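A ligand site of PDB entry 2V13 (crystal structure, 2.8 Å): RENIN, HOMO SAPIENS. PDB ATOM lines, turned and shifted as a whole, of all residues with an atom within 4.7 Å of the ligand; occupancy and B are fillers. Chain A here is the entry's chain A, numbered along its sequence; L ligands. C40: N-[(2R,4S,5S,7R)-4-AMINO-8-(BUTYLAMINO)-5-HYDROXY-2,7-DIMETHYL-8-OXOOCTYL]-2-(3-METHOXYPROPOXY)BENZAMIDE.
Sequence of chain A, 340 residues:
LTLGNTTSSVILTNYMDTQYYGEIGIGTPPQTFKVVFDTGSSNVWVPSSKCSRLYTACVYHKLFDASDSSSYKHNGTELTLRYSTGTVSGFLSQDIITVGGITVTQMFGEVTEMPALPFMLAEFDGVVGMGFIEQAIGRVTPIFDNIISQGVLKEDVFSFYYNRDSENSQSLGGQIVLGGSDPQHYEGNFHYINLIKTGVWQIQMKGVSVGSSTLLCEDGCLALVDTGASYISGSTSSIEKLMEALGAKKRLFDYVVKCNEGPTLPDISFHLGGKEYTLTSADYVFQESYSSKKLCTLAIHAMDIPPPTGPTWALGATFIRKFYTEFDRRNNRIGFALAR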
ATOM      1  N   THR A  18     -13.997 -17.996   4.353  1.00  0.00           N
ATOM      2  CA  THR A  18     -12.741 -18.640   4.415  1.00  0.00           C
ATOM      3  C   THR A  18     -12.899 -20.090   4.107  1.00  0.00           C
ATOM      4  O   THR A  18     -11.895 -20.772   4.173  1.00  0.00           O
ATOM      5  CB  THR A  18     -12.117 -18.435   5.809  1.00  0.00           C
ATOM      6  OG1 THR A  18     -13.027 -18.865   6.787  1.00  0.00           O
ATOM      7  CG2 THR A  18     -11.787 -17.011   6.067  1.00  0.00           C
ATOM      8  N   GLN A  19     -14.038 -20.622   3.672  1.00  0.00           N
ATOM      9  CA  GLN A  19     -14.175 -22.054   3.589  1.00  0.00           C
ATOM     10  C   GLN A  19     -15.379 -22.330   2.752  1.00  0.00           C
ATOM     11  O   GLN A  19     -16.457 -21.917   3.165  1.00  0.00           O
ATOM     12  CB  GLN A  19     -14.363 -22.474   4.995  1.00  0.00           C
ATOM     13  CG  GLN A  19     -14.379 -23.904   5.331  1.00  0.00           C
ATOM     14  CD  GLN A  19     -13.879 -24.105   6.750  1.00  0.00           C
ATOM     15  OE1 GLN A  19     -14.483 -24.899   7.462  1.00  0.00           O
ATOM     16  NE2 GLN A  19     -12.841 -23.525   7.332  1.00  0.00           N
ATOM     17  N   TYR A  20     -15.231 -22.932   1.582  1.00  0.00           N
ATOM     18  CA  TYR A  20     -16.370 -23.192   0.712  1.00  0.00           C
ATOM     19  C   TYR A  20     -16.401 -24.668   0.402  1.00  0.00           C
ATOM     20  O   TYR A  20     -15.399 -25.223  -0.029  1.00  0.00           O
ATOM     21  CB  TYR A  20     -16.272 -22.453  -0.613  1.00  0.00           C
ATOM     22  CG  TYR A  20     -16.208 -20.929  -0.584  1.00  0.00           C
ATOM     23  CD1 TYR A  20     -15.279 -20.282   0.158  1.00  0.00           C
ATOM     24  CD2 TYR A  20     -17.136 -20.237  -1.305  1.00  0.00           C
ATOM     25  CE1 TYR A  20     -15.285 -18.923   0.193  1.00  0.00           C
ATOM     26  CE2 TYR A  20     -17.152 -18.877  -1.270  1.00  0.00           C
ATOM     27  CZ  TYR A  20     -16.234 -18.237  -0.524  1.00  0.00           C
ATOM     28  OH  TYR A  20     -16.276 -16.882  -0.397  1.00  0.00           O
ATOM     29  N   VAL A  36     -14.463 -30.352   0.153  1.00  0.00           N
ATOM     30  CA  VAL A  36     -13.979 -29.183  -0.494  1.00  0.00           C
ATOM     31  C   VAL A  36     -13.627 -29.619  -1.886  1.00  0.00           C
ATOM     32  O   VAL A  36     -13.027 -30.658  -2.087  1.00  0.00           O
ATOM     33  CB  VAL A  36     -12.740 -28.699   0.206  1.00  0.00           C
ATOM     34  CG1 VAL A  36     -12.134 -27.551  -0.502  1.00  0.00           C
ATOM     35  CG2 VAL A  36     -13.124 -28.070   1.493  1.00  0.00           C
ATOM     36  N   ASP A  38     -11.199 -29.308  -4.285  1.00  0.00           N
ATOM     37  CA  ASP A  38      -9.864 -28.734  -4.346  1.00  0.00           C
ATOM     38  C   ASP A  38      -9.090 -28.764  -5.640  1.00  0.00           C
ATOM     39  O   ASP A  38      -8.655 -29.859  -5.997  1.00  0.00           O
ATOM     40  CB  ASP A  38      -9.075 -29.423  -3.287  1.00  0.00           C
ATOM     41  CG  ASP A  38      -7.672 -28.932  -2.986  1.00  0.00           C
ATOM     42  OD1 ASP A  38      -7.294 -27.815  -3.347  1.00  0.00           O
ATOM     43  OD2 ASP A  38      -6.968 -29.702  -2.331  1.00  0.00           O
ATOM     44  N   GLY A  40      -6.064 -28.425  -6.167  1.00  0.00           N
ATOM     45  CA  GLY A  40      -4.630 -28.488  -6.007  1.00  0.00           C
ATOM     46  C   GLY A  40      -4.191 -29.836  -5.526  1.00  0.00           C
ATOM     47  O   GLY A  40      -3.037 -29.907  -5.085  1.00  0.00           O
ATOM     48  N   SER A  41      -5.075 -30.862  -5.505  1.00  0.00           N
ATOM     49  CA  SER A  41      -4.713 -32.196  -5.073  1.00  0.00           C
ATOM     50  C   SER A  41      -5.510 -33.148  -5.871  1.00  0.00           C
ATOM     51  O   SER A  41      -6.467 -32.710  -6.499  1.00  0.00           O
ATOM     52  CB  SER A  41      -5.050 -32.413  -3.640  1.00  0.00           C
ATOM     53  OG  SER A  41      -6.306 -33.039  -3.311  1.00  0.00           O
ATOM     54  N   LEU A  81      -1.362 -38.784   2.710  1.00  0.00           N
ATOM     55  CA  LEU A  81      -1.542 -37.556   1.934  1.00  0.00           C
ATOM     56  C   LEU A  81      -1.019 -36.383   2.700  1.00  0.00           C
ATOM     57  O   LEU A  81      -1.452 -35.980   3.787  1.00  0.00           O
ATOM     58  CB  LEU A  81      -3.017 -37.253   1.624  1.00  0.00           C
ATOM     59  CG  LEU A  81      -3.845 -38.419   1.066  1.00  0.00           C
ATOM     60  CD1 LEU A  81      -4.628 -38.936   2.239  1.00  0.00           C
ATOM     61  CD2 LEU A  81      -4.898 -38.061   0.057  1.00  0.00           C
ATOM     62  N   ARG A  82      -0.073 -35.848   1.969  1.00  0.00           N
ATOM     63  CA  ARG A  82       0.656 -34.778   2.544  1.00  0.00           C
ATOM     64  C   ARG A  82       0.238 -33.447   1.993  1.00  0.00           C
ATOM     65  O   ARG A  82       0.909 -32.835   1.146  1.00  0.00           O
ATOM     66  CB  ARG A  82       2.101 -35.026   2.271  1.00  0.00           C
ATOM     67  CG  ARG A  82       2.695 -35.727   3.498  1.00  0.00           C
ATOM     68  CD  ARG A  82       4.123 -36.272   3.327  1.00  0.00           C
ATOM     69  NE  ARG A  82       4.377 -36.999   4.567  1.00  0.00           N
ATOM     70  CZ  ARG A  82       4.556 -38.339   4.595  1.00  0.00           C
ATOM     71  NH1 ARG A  82       4.541 -39.108   3.457  1.00  0.00           N
ATOM     72  NH2 ARG A  82       4.720 -38.883   5.849  1.00  0.00           N
ATOM     73  N   TYR A  83      -0.882 -32.963   2.485  1.00  0.00           N
ATOM     74  CA  TYR A  83      -1.267 -31.669   1.963  1.00  0.00           C
ATOM     75  C   TYR A  83      -0.255 -30.676   2.499  1.00  0.00           C
ATOM     76  O   TYR A  83       0.312 -30.889   3.577  1.00  0.00           O
ATOM     77  CB  TYR A  83      -2.693 -31.372   2.435  1.00  0.00           C
ATOM     78  CG  TYR A  83      -3.750 -32.252   1.789  1.00  0.00           C
ATOM     79  CD1 TYR A  83      -4.064 -32.063   0.469  1.00  0.00           C
ATOM     80  CD2 TYR A  83      -4.358 -33.237   2.505  1.00  0.00           C
ATOM     81  CE1 TYR A  83      -5.002 -32.883  -0.121  1.00  0.00           C
ATOM     82  CE2 TYR A  83      -5.285 -34.054   1.924  1.00  0.00           C
ATOM     83  CZ  TYR A  83      -5.599 -33.860   0.614  1.00  0.00           C
ATOM     84  OH  TYR A  83      -6.578 -34.623   0.030  1.00  0.00           O
ATOM     85  N   SER A  84      -0.014 -29.581   1.785  1.00  0.00           N
ATOM     86  CA  SER A  84       0.738 -28.447   2.317  1.00  0.00           C
ATOM     87  C   SER A  84       0.259 -27.984   3.689  1.00  0.00           C
ATOM     88  O   SER A  84       0.887 -27.091   4.232  1.00  0.00           O
ATOM     89  CB  SER A  84       0.609 -27.236   1.481  1.00  0.00           C
ATOM     90  OG  SER A  84      -0.707 -26.725   1.721  1.00  0.00           O
ATOM     91  N   THR A  85      -0.902 -28.356   4.224  1.00  0.00           N
ATOM     92  CA  THR A  85      -1.290 -27.914   5.547  1.00  0.00           C
ATOM     93  C   THR A  85      -1.367 -29.017   6.605  1.00  0.00           C
ATOM     94  O   THR A  85      -1.708 -28.758   7.782  1.00  0.00           O
ATOM     95  CB  THR A  85      -2.591 -27.211   5.380  1.00  0.00           C
ATOM     96  OG1 THR A  85      -3.507 -28.200   4.983  1.00  0.00           O
ATOM     97  CG2 THR A  85      -2.578 -26.209   4.251  1.00  0.00           C
ATOM     98  N   PRO A 118      -4.918 -28.707  11.000  1.00  0.00           N
ATOM     99  CA  PRO A 118      -6.042 -27.838  11.125  1.00  0.00           C
ATOM    100  C   PRO A 118      -7.339 -28.540  10.990  1.00  0.00           C
ATOM    101  O   PRO A 118      -8.375 -27.872  11.088  1.00  0.00           O
ATOM    102  CB  PRO A 118      -5.867 -26.870  10.063  1.00  0.00           C
ATOM    103  CG  PRO A 118      -5.491 -27.835   8.963  1.00  0.00           C
ATOM    104  CD  PRO A 118      -4.540 -28.825   9.596  1.00  0.00           C
ATOM    105  N   PHE A 119      -7.389 -29.860  10.804  1.00  0.00           N
ATOM    106  CA  PHE A 119      -8.683 -30.415  10.531  1.00  0.00           C
ATOM    107  C   PHE A 119      -9.675 -30.186  11.612  1.00  0.00           C
ATOM    108  O   PHE A 119     -10.853 -30.308  11.367  1.00  0.00           O
ATOM    109  CB  PHE A 119      -8.527 -31.862  10.245  1.00  0.00           C
ATOM    110  CG  PHE A 119      -7.908 -31.877   8.871  1.00  0.00           C
ATOM    111  CD1 PHE A 119      -8.702 -31.687   7.768  1.00  0.00           C
ATOM    112  CD2 PHE A 119      -6.555 -32.028   8.731  1.00  0.00           C
ATOM    113  CE1 PHE A 119      -8.128 -31.636   6.508  1.00  0.00           C
ATOM    114  CE2 PHE A 119      -6.021 -31.974   7.460  1.00  0.00           C
ATOM    115  CZ  PHE A 119      -6.782 -31.781   6.332  1.00  0.00           C
ATOM    116  N   LEU A 121     -10.318 -27.217  12.728  1.00  0.00           N
ATOM    117  CA  LEU A 121     -11.075 -26.001  12.446  1.00  0.00           C
ATOM    118  C   LEU A 121     -11.895 -26.186  11.171  1.00  0.00           C
ATOM    119  O   LEU A 121     -12.286 -25.181  10.568  1.00  0.00           O
ATOM    120  CB  LEU A 121     -10.256 -24.789  12.156  1.00  0.00           C
ATOM    121  CG  LEU A 121      -9.027 -24.362  12.852  1.00  0.00           C
ATOM    122  CD1 LEU A 121      -9.097 -24.680  14.281  1.00  0.00           C
ATOM    123  CD2 LEU A 121      -7.867 -25.019  12.165  1.00  0.00           C
ATOM    124  N   ALA A 122     -12.244 -27.374  10.719  1.00  0.00           N
ATOM    125  CA  ALA A 122     -12.914 -27.400   9.462  1.00  0.00           C
ATOM    126  C   ALA A 122     -14.299 -27.910   9.515  1.00  0.00           C
ATOM    127  O   ALA A 122     -14.503 -29.081   9.863  1.00  0.00           O
ATOM    128  CB  ALA A 122     -12.153 -28.261   8.521  1.00  0.00           C
ATOM    129  N   PHE A 124     -15.797 -28.705   6.903  1.00  0.00           N
ATOM    130  CA  PHE A 124     -16.133 -29.649   5.873  1.00  0.00           C
ATOM    131  C   PHE A 124     -15.767 -30.981   6.426  1.00  0.00           C
ATOM    132  O   PHE A 124     -15.422 -30.983   7.609  1.00  0.00           O
ATOM    133  CB  PHE A 124     -15.356 -29.362   4.624  1.00  0.00           C
ATOM    134  CG  PHE A 124     -13.886 -29.113   4.764  1.00  0.00           C
ATOM    135  CD1 PHE A 124     -12.995 -30.150   4.641  1.00  0.00           C
ATOM    136  CD2 PHE A 124     -13.438 -27.836   4.979  1.00  0.00           C
ATOM    137  CE1 PHE A 124     -11.646 -29.911   4.733  1.00  0.00           C
ATOM    138  CE2 PHE A 124     -12.095 -27.633   5.067  1.00  0.00           C
ATOM    139  CZ  PHE A 124     -11.192 -28.658   4.949  1.00  0.00           C
ATOM    140  N   VAL A 127     -12.462 -34.147   1.191  1.00  0.00           N
ATOM    141  CA  VAL A 127     -11.864 -33.308   0.178  1.00  0.00           C
ATOM    142  C   VAL A 127     -12.092 -34.115  -1.100  1.00  0.00           C
ATOM    143  O   VAL A 127     -12.062 -35.356  -1.004  1.00  0.00           O
ATOM    144  CB  VAL A 127     -10.373 -33.141   0.413  1.00  0.00           C
ATOM    145  CG1 VAL A 127      -9.804 -32.404  -0.771  1.00  0.00           C
ATOM    146  CG2 VAL A 127     -10.066 -32.356   1.656  1.00  0.00           C
ATOM    147  N   ILE A 137      -2.306 -39.298  -5.266  1.00  0.00           N
ATOM    148  CA  ILE A 137      -1.500 -40.214  -4.520  1.00  0.00           C
ATOM    149  C   ILE A 137      -2.286 -41.482  -4.650  1.00  0.00           C
ATOM    150  O   ILE A 137      -3.519 -41.525  -4.553  1.00  0.00           O
ATOM    151  CB  ILE A 137      -1.387 -39.783  -3.086  1.00  0.00           C
ATOM    152  CG1 ILE A 137      -0.230 -38.861  -3.044  1.00  0.00           C
ATOM    153  CG2 ILE A 137      -1.138 -40.907  -2.118  1.00  0.00           C
ATOM    154  CD1 ILE A 137      -0.053 -38.296  -1.611  1.00  0.00           C
ATOM    155  N   TYR A 162     -17.413 -18.257  -6.237  1.00  0.00           N
ATOM    156  CA  TYR A 162     -17.390 -18.278  -4.812  1.00  0.00           C
ATOM    157  C   TYR A 162     -17.999 -16.966  -4.477  1.00  0.00           C
ATOM    158  O   TYR A 162     -17.462 -15.922  -4.808  1.00  0.00           O
ATOM    159  CB  TYR A 162     -16.036 -18.302  -4.334  1.00  0.00           C
ATOM    160  CG  TYR A 162     -15.414 -19.657  -4.269  1.00  0.00           C
ATOM    161  CD1 TYR A 162     -16.057 -20.840  -4.535  1.00  0.00           C
ATOM    162  CD2 TYR A 162     -14.127 -19.678  -3.879  1.00  0.00           C
ATOM    163  CE1 TYR A 162     -15.402 -22.046  -4.410  1.00  0.00           C
ATOM    164  CE2 TYR A 162     -13.468 -20.862  -3.755  1.00  0.00           C
ATOM    165  CZ  TYR A 162     -14.098 -22.029  -4.006  1.00  0.00           C
ATOM    166  OH  TYR A 162     -13.385 -23.187  -3.852  1.00  0.00           O
ATOM    167  N   LEU A 224      -0.383 -21.178  -8.297  1.00  0.00           N
ATOM    168  CA  LEU A 224      -1.262 -22.317  -8.342  1.00  0.00           C
ATOM    169  C   LEU A 224      -2.634 -21.750  -8.194  1.00  0.00           C
ATOM    170  O   LEU A 224      -2.879 -21.016  -7.254  1.00  0.00           O
ATOM    171  CB  LEU A 224      -0.875 -23.190  -7.224  1.00  0.00           C
ATOM    172  CG  LEU A 224      -1.640 -24.465  -7.017  1.00  0.00           C
ATOM    173  CD1 LEU A 224      -1.896 -25.144  -8.302  1.00  0.00           C
ATOM    174  CD2 LEU A 224      -0.794 -25.451  -6.305  1.00  0.00           C
ATOM    175  N   ASP A 226      -5.833 -22.254  -6.678  1.00  0.00           N
ATOM    176  CA  ASP A 226      -6.237 -23.370  -5.825  1.00  0.00           C
ATOM    177  C   ASP A 226      -7.539 -23.220  -5.118  1.00  0.00           C
ATOM    178  O   ASP A 226      -7.574 -22.797  -3.987  1.00  0.00           O
ATOM    179  CB  ASP A 226      -5.118 -23.544  -4.875  1.00  0.00           C
ATOM    180  CG  ASP A 226      -5.253 -24.407  -3.655  1.00  0.00           C
ATOM    181  OD1 ASP A 226      -4.410 -24.218  -2.796  1.00  0.00           O
ATOM    182  OD2 ASP A 226      -6.153 -25.212  -3.540  1.00  0.00           O
ATOM    183  N   THR A 227      -8.612 -23.753  -5.644  1.00  0.00           N
ATOM    184  CA  THR A 227      -9.937 -23.602  -5.082  1.00  0.00           C
ATOM    185  C   THR A 227     -10.044 -24.081  -3.672  1.00  0.00           C
ATOM    186  O   THR A 227     -10.991 -23.816  -2.956  1.00  0.00           O
ATOM    187  CB  THR A 227     -10.896 -24.380  -5.893  1.00  0.00           C
ATOM    188  OG1 THR A 227     -10.495 -25.744  -5.916  1.00  0.00           O
ATOM    189  CG2 THR A 227     -10.918 -23.828  -7.301  1.00  0.00           C
ATOM    190  N   GLY A 228      -9.075 -24.877  -3.303  1.00  0.00           N
ATOM    191  CA  GLY A 228      -9.041 -25.321  -1.971  1.00  0.00           C
ATOM    192  C   GLY A 228      -8.048 -24.486  -1.212  1.00  0.00           C
ATOM    193  O   GLY A 228      -7.079 -25.074  -0.722  1.00  0.00           O
ATOM    194  N   ALA A 229      -8.165 -23.176  -1.161  1.00  0.00           N
ATOM    195  CA  ALA A 229      -7.347 -22.369  -0.281  1.00  0.00           C
ATOM    196  C   ALA A 229      -8.100 -21.087   0.162  1.00  0.00           C
ATOM    197  O   ALA A 229      -8.780 -20.456  -0.648  1.00  0.00           O
ATOM    198  CB  ALA A 229      -6.119 -22.025  -1.028  1.00  0.00           C
ATOM    199  N   SER A 230      -8.111 -20.560   1.375  1.00  0.00           N
ATOM    200  CA  SER A 230      -8.962 -19.422   1.648  1.00  0.00           C
ATOM    201  C   SER A 230      -8.421 -18.115   1.165  1.00  0.00           C
ATOM    202  O   SER A 230      -9.228 -17.217   0.952  1.00  0.00           O
ATOM    203  CB  SER A 230      -9.169 -19.299   3.110  1.00  0.00           C
ATOM    204  OG  SER A 230      -9.134 -20.582   3.740  1.00  0.00           O
ATOM    205  N   ILE A 305       4.709 -23.498  -0.152  1.00  0.00           N
ATOM    206  CA  ILE A 305       4.332 -24.767  -0.708  1.00  0.00           C
ATOM    207  C   ILE A 305       5.646 -25.385  -1.096  1.00  0.00           C
ATOM    208  O   ILE A 305       6.518 -24.698  -1.642  1.00  0.00           O
ATOM    209  CB  ILE A 305       3.502 -24.587  -1.938  1.00  0.00           C
ATOM    210  CG1 ILE A 305       2.158 -24.186  -1.521  1.00  0.00           C
ATOM    211  CG2 ILE A 305       3.412 -25.863  -2.758  1.00  0.00           C
ATOM    212  CD1 ILE A 305       1.663 -23.214  -2.573  1.00  0.00           C
ATOM    213  N   THR A 309       5.397 -28.979  -6.311  1.00  0.00           N
ATOM    214  CA  THR A 309       4.323 -28.213  -6.918  1.00  0.00           C
ATOM    215  C   THR A 309       4.837 -26.810  -6.767  1.00  0.00           C
ATOM    216  O   THR A 309       4.796 -26.059  -7.714  1.00  0.00           O
ATOM    217  CB  THR A 309       2.928 -28.250  -6.216  1.00  0.00           C
ATOM    218  OG1 THR A 309       2.650 -26.985  -5.591  1.00  0.00           O
ATOM    219  CG2 THR A 309       2.882 -29.346  -5.152  1.00  0.00           C
HETATM  220  C1  C40 L   1     -12.407 -23.368  -0.218  1.00  0.00           C
HETATM  221  O2  C40 L   1     -12.502 -23.314   1.196  1.00  0.00           O
HETATM  222  C3  C40 L   1     -11.729 -24.415   1.555  1.00  0.00           C
HETATM  223  C4  C40 L   1     -10.517 -23.895   2.295  1.00  0.00           C
HETATM  224  C5  C40 L   1     -10.183 -25.079   3.177  1.00  0.00           C
HETATM  225  O6  C40 L   1      -8.911 -25.008   3.790  1.00  0.00           O
HETATM  226  C7  C40 L   1      -8.708 -25.559   5.046  1.00  0.00           C
HETATM  227  C8  C40 L   1      -9.508 -25.018   6.034  1.00  0.00           C
HETATM  228  C9  C40 L   1      -9.556 -25.547   7.299  1.00  0.00           C
HETATM  229  C10 C40 L   1      -8.806 -26.631   7.571  1.00  0.00           C
HETATM  230  C11 C40 L   1      -7.998 -27.182   6.611  1.00  0.00           C
HETATM  231  C12 C40 L   1      -7.923 -26.671   5.343  1.00  0.00           C
HETATM  232  C13 C40 L   1      -7.079 -27.243   4.380  1.00  0.00           C
HETATM  233  O14 C40 L   1      -5.899 -27.344   4.611  1.00  0.00           O
HETATM  234  C16 C40 L   1      -6.422 -27.257   2.090  1.00  0.00           C
HETATM  235  N15 C40 L   1      -7.439 -27.296   3.125  1.00  0.00           N
HETATM  236  C18 C40 L   1      -7.651 -29.448   1.659  1.00  0.00           C
HETATM  237  C17 C40 L   1      -6.841 -28.255   1.079  1.00  0.00           C
HETATM  238  C19 C40 L   1      -5.613 -28.811   0.418  1.00  0.00           C
HETATM  239  N21 C40 L   1      -5.477 -26.928  -1.081  1.00  0.00           N
HETATM  240  C20 C40 L   1      -4.736 -27.843  -0.245  1.00  0.00           C
HETATM  241  C22 C40 L   1      -3.798 -28.663  -1.122  1.00  0.00           C
HETATM  242  O23 C40 L   1      -4.551 -28.683  -2.335  1.00  0.00           O
HETATM  243  C24 C40 L   1      -2.410 -28.024  -1.395  1.00  0.00           C
HETATM  244  C25 C40 L   1      -1.619 -28.703  -2.482  1.00  0.00           C
HETATM  245  C26 C40 L   1      -0.501 -27.870  -2.952  1.00  0.00           C
HETATM  246  C27 C40 L   1      -0.982 -29.995  -2.103  1.00  0.00           C
HETATM  247  O28 C40 L   1      -0.640 -30.188  -0.938  1.00  0.00           O
HETATM  248  C30 C40 L   1      -0.343 -32.218  -2.771  1.00  0.00           C
HETATM  249  N29 C40 L   1      -0.779 -30.858  -3.068  1.00  0.00           N
HETATM  250  C31 C40 L   1      -1.405 -32.996  -2.007  1.00  0.00           C
HETATM  251  C32 C40 L   1      -1.150 -34.494  -2.015  1.00  0.00           C
HETATM  252  C33 C40 L   1       0.150 -34.843  -1.230  1.00  0.00           C
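The side-chain carboxylate (OD1) of Asp 38 sits close to the backbone NH (N) of Gly 40 (3.1 Å).
The side-chain hydroxyl of Ser 230 is in hydrogen-bond range of the backbone carbonyl oxygen of Thr 18, 2.8 Å away.
OD2 of Asp 226 sits close to N of Gly 228 (3.0 Å).
The backbone NH of Gly 228 sits close to the side-chain carboxylate of Asp 38, at 3.4 Å.
The backbone carbonyl oxygen (O) of Thr 227 lies within hydrogen-bond range of the side-chain hydroxyl (OH) of Tyr 162 (2.6 Å).
N of Tyr 20 sits at hydrogen-bond distance from O2 of the ligand.
O28 of the ligand lies within hydrogen-bond range of N of Ser 84 (2.9 Å).
The side-chain carboxylate (OD1) of Asp 38 is in salt-bridge range of a nitrogen (N21) of the ligand.
O of Gly 40 sits at hydrogen-bond distance from N29 of the ligand, 3.2 Å away.
A nitrogen (N21) of the ligand is in hydrogen-bond range of the backbone carbonyl oxygen of Gly 228.
The side-chain carboxylate (OD2) of Asp 226 is in salt-bridge range of a nitrogen (N21) of the ligand (3.1 Å).
The side-chain hydroxyl of Thr 85 is in hydrogen-bond range of an oxygen (O14) of the ligand (2.6 Å).
O of Thr 18 touches C4 of the ligand, 3.9 Å away.
CA of Gln 19 touches O2 of the ligand, 3.2 Å away.
CG1 of Val 36 touches C3 of the ligand, 3.8 Å away.
N of Ser 41 touches O23 of the ligand, at 3.9 Å.
Arg 82 touches the ligand.
Tyr 83 touches the ligand (CA to O28, 3.3 Å).
Pro 118 touches the ligand (CG to C11, 3.5 Å).
Ala 122 touches the ligand.
Phe 124 touches the ligand (CE2 to C5, 3.7 Å).
Val 127 touches the ligand (CG2 to C18, 3.8 Å).
Ile 137 touches the ligand.
Tyr 162 touches the ligand.
Thr 227 touches the ligand.
Ser 230 touches the ligand.
Hydrophobic or aromatic side chains within 4 Å of the ligand: Tyr 20, Val 36, Tyr 83, Pro 118, Ala 122, Phe 124, Val 127 and Ile 137.
Within 4 Å of the ligand: Thr 18, Gln 19, Tyr 20, Val 36, Asp 38, Gly 40, Ser 41, Arg 82, Tyr 83, Ser 84, Thr 85, Pro 118, Ala 122, Phe 124, Val 127, Ile 137, Tyr 162, Asp 226, Thr 227, Gly 228 and Ser 230.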
